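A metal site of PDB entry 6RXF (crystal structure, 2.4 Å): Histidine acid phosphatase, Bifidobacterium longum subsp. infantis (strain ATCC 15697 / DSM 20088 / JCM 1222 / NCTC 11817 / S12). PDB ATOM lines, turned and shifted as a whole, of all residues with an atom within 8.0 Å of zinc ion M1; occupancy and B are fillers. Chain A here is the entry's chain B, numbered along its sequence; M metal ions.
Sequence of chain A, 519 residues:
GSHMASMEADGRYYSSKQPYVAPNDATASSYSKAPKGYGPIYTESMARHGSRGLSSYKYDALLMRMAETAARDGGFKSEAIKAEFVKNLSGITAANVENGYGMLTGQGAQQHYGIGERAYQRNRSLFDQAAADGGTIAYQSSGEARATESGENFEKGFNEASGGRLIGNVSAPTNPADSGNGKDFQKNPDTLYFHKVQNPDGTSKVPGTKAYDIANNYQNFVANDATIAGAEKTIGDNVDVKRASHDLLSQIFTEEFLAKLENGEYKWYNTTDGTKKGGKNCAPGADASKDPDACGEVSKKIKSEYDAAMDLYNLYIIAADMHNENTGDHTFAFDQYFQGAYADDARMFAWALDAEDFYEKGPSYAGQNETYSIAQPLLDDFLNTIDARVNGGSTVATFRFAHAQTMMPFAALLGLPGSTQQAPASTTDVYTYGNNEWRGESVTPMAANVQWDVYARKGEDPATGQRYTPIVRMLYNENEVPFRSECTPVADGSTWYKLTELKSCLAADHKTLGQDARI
OE1 of Glu 360 is in salt-bridge range of NZ of Lys 361 (2.8 Å).
Within 4 Å of zinc ion M1: Glu 232, Glu 356 and Glu 360.
Zinc ion M1 is bound by OE2 of Glu 356 (2.0 Å), OE2 of Glu 360 (2.3 Å) and OE2 of Glu 232 (2.4 Å).
Zinc ion M1 has three donor atoms within binding distance.
Slightly farther from zinc ion M1 lies the side-chain carboxylate (OE1) of Glu 232 (2.8 Å).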
ATOM      1  N   VAL A 222      13.142   9.161  -5.902  1.00  0.00           N
ATOM      2  CA  VAL A 222      14.575   9.366  -6.099  1.00  0.00           C
ATOM      3  C   VAL A 222      15.386   8.531  -5.119  1.00  0.00           C
ATOM      4  O   VAL A 222      16.418   7.951  -5.485  1.00  0.00           O
ATOM      5  CB  VAL A 222      14.909  10.873  -5.994  1.00  0.00           C
ATOM      6  CG1 VAL A 222      16.363  11.082  -5.622  1.00  0.00           C
ATOM      7  CG2 VAL A 222      14.613  11.551  -7.319  1.00  0.00           C
ATOM      8  N   ALA A 223      14.941   8.426  -3.870  1.00  0.00           N
ATOM      9  CA  ALA A 223      15.688   7.654  -2.880  1.00  0.00           C
ATOM     10  C   ALA A 223      15.644   6.159  -3.148  1.00  0.00           C
ATOM     11  O   ALA A 223      16.538   5.434  -2.682  1.00  0.00           O
ATOM     12  CB  ALA A 223      15.165   7.952  -1.476  1.00  0.00           C
ATOM     13  N   ILE A 228      18.156   4.540 -11.352  1.00  0.00           N
ATOM     14  CA  ILE A 228      19.030   5.646 -10.960  1.00  0.00           C
ATOM     15  C   ILE A 228      20.166   5.130 -10.090  1.00  0.00           C
ATOM     16  O   ILE A 228      21.335   5.498 -10.287  1.00  0.00           O
ATOM     17  CB  ILE A 228      18.216   6.742 -10.243  1.00  0.00           C
ATOM     18  CG1 ILE A 228      17.260   7.429 -11.214  1.00  0.00           C
ATOM     19  CG2 ILE A 228      19.157   7.759  -9.602  1.00  0.00           C
ATOM     20  CD1 ILE A 228      16.230   8.316 -10.546  1.00  0.00           C
ATOM     21  N   ALA A 229      19.857   4.275  -9.119  1.00  0.00           N
ATOM     22  CA  ALA A 229      20.870   3.755  -8.216  1.00  0.00           C
ATOM     23  C   ALA A 229      21.943   2.975  -8.973  1.00  0.00           C
ATOM     24  O   ALA A 229      23.134   3.099  -8.675  1.00  0.00           O
ATOM     25  CB  ALA A 229      20.222   2.861  -7.151  1.00  0.00           C
ATOM     26  N   GLU A 232      24.093   5.453 -11.200  1.00  0.00           N
ATOM     27  CA  GLU A 232      25.029   6.235 -10.404  1.00  0.00           C
ATOM     28  C   GLU A 232      26.151   5.375  -9.834  1.00  0.00           C
ATOM     29  O   GLU A 232      27.279   5.842  -9.662  1.00  0.00           O
ATOM     30  CB  GLU A 232      24.288   6.949  -9.272  1.00  0.00           C
ATOM     31  CG  GLU A 232      23.544   8.218  -9.731  1.00  0.00           C
ATOM     32  CD  GLU A 232      23.167   9.143  -8.599  1.00  0.00           C
ATOM     33  OE1 GLU A 232      23.761  10.235  -8.503  1.00  0.00           O
ATOM     34  OE2 GLU A 232      22.263   8.780  -7.811  1.00  0.00           O
ATOM     35  N   LYS A 233      25.849   4.111  -9.522  1.00  0.00           N
ATOM     36  CA  LYS A 233      26.909   3.187  -9.142  1.00  0.00           C
ATOM     37  C   LYS A 233      27.881   2.972 -10.298  1.00  0.00           C
ATOM     38  O   LYS A 233      29.100   2.941 -10.093  1.00  0.00           O
ATOM     39  CB  LYS A 233      26.293   1.857  -8.696  1.00  0.00           C
ATOM     40  CG  LYS A 233      27.248   0.941  -7.959  1.00  0.00           C
ATOM     41  CD  LYS A 233      27.477  -0.370  -8.715  1.00  0.00           C
ATOM     42  CE  LYS A 233      28.238  -1.378  -7.857  1.00  0.00           C
ATOM     43  NZ  LYS A 233      29.545  -0.830  -7.366  1.00  0.00           N
ATOM     44  N   ALA A 355      26.087  14.232 -14.134  1.00  0.00           N
ATOM     45  CA  ALA A 355      25.372  12.973 -14.168  1.00  0.00           C
ATOM     46  C   ALA A 355      24.362  12.857 -13.031  1.00  0.00           C
ATOM     47  O   ALA A 355      23.188  12.534 -13.254  1.00  0.00           O
ATOM     48  CB  ALA A 355      26.358  11.801 -14.152  1.00  0.00           C
ATOM     49  N   GLU A 356      24.803  13.134 -11.791  1.00  0.00           N
ATOM     50  CA  GLU A 356      23.900  13.064 -10.639  1.00  0.00           C
ATOM     51  C   GLU A 356      22.712  14.007 -10.798  1.00  0.00           C
ATOM     52  O   GLU A 356      21.559  13.650 -10.524  1.00  0.00           O
ATOM     53  CB  GLU A 356      24.660  13.386  -9.349  1.00  0.00           C
ATOM     54  CG  GLU A 356      23.731  13.600  -8.148  1.00  0.00           C
ATOM     55  OE1 GLU A 356      25.347  12.721  -6.655  1.00  0.00           O
ATOM     56  OE2 GLU A 356      23.252  12.231  -6.278  1.00  0.00           O
ATOM     57  N   ASP A 357      23.019  15.242 -11.200  1.00  0.00           N
ATOM     58  CA  ASP A 357      21.969  16.219 -11.476  1.00  0.00           C
ATOM     59  C   ASP A 357      21.049  15.744 -12.606  1.00  0.00           C
ATOM     60  O   ASP A 357      19.820  15.858 -12.496  1.00  0.00           O
ATOM     61  CB  ASP A 357      22.598  17.565 -11.821  1.00  0.00           C
ATOM     62  CG  ASP A 357      22.815  18.437 -10.596  1.00  0.00           C
ATOM     63  OD1 ASP A 357      22.133  18.211  -9.587  1.00  0.00           O
ATOM     64  OD2 ASP A 357      23.647  19.379 -10.658  1.00  0.00           O
ATOM     65  N   TYR A 359      20.288  12.701 -13.675  1.00  0.00           N
ATOM     66  CA  TYR A 359      19.434  11.576 -13.328  1.00  0.00           C
ATOM     67  C   TYR A 359      18.418  11.913 -12.243  1.00  0.00           C
ATOM     68  O   TYR A 359      17.391  11.226 -12.157  1.00  0.00           O
ATOM     69  CB  TYR A 359      20.270  10.393 -12.852  1.00  0.00           C
ATOM     70  CG  TYR A 359      20.848   9.554 -13.970  1.00  0.00           C
ATOM     71  CD1 TYR A 359      20.024   8.791 -14.795  1.00  0.00           C
ATOM     72  CD2 TYR A 359      22.209   9.538 -14.215  1.00  0.00           C
ATOM     73  CE1 TYR A 359      20.545   8.029 -15.816  1.00  0.00           C
ATOM     74  CE2 TYR A 359      22.746   8.787 -15.228  1.00  0.00           C
ATOM     75  CZ  TYR A 359      21.911   8.036 -16.028  1.00  0.00           C
ATOM     76  OH  TYR A 359      22.461   7.283 -17.038  1.00  0.00           O
ATOM     77  N   GLU A 360      18.654  12.940 -11.429  1.00  0.00           N
ATOM     78  CA  GLU A 360      17.779  13.213 -10.300  1.00  0.00           C
ATOM     79  C   GLU A 360      16.835  14.387 -10.529  1.00  0.00           C
ATOM     80  O   GLU A 360      15.727  14.380  -9.989  1.00  0.00           O
ATOM     81  CB  GLU A 360      18.614  13.472  -9.040  1.00  0.00           C
ATOM     82  CG  GLU A 360      19.385  12.248  -8.565  1.00  0.00           C
ATOM     83  CD  GLU A 360      20.095  12.484  -7.248  1.00  0.00           C
ATOM     84  OE1 GLU A 360      20.183  13.652  -6.817  1.00  0.00           O
ATOM     85  OE2 GLU A 360      20.558  11.491  -6.644  1.00  0.00           O
ATOM     86  N   LYS A 361      17.247  15.381 -11.311  1.00  0.00           N
ATOM     87  CA  LYS A 361      16.418  16.555 -11.530  1.00  0.00           C
ATOM     88  C   LYS A 361      16.183  16.877 -12.993  1.00  0.00           C
ATOM     89  O   LYS A 361      15.354  17.751 -13.287  1.00  0.00           O
ATOM     90  CB  LYS A 361      17.029  17.788 -10.840  1.00  0.00           C
ATOM     91  CG  LYS A 361      17.269  17.621  -9.342  1.00  0.00           C
ATOM     92  CD  LYS A 361      18.759  17.604  -9.013  1.00  0.00           C
ATOM     93  CE  LYS A 361      19.005  17.430  -7.516  1.00  0.00           C
ATOM     94  NZ  LYS A 361      18.724  16.041  -7.039  1.00  0.00           N
HETATM   95 ZN    ZN M   1      22.439  10.387  -5.986  1.00  0.00          ZN
HETATM   96 ZN    ZN M   2      20.905   7.663  -5.294  1.00  0.00          ZN
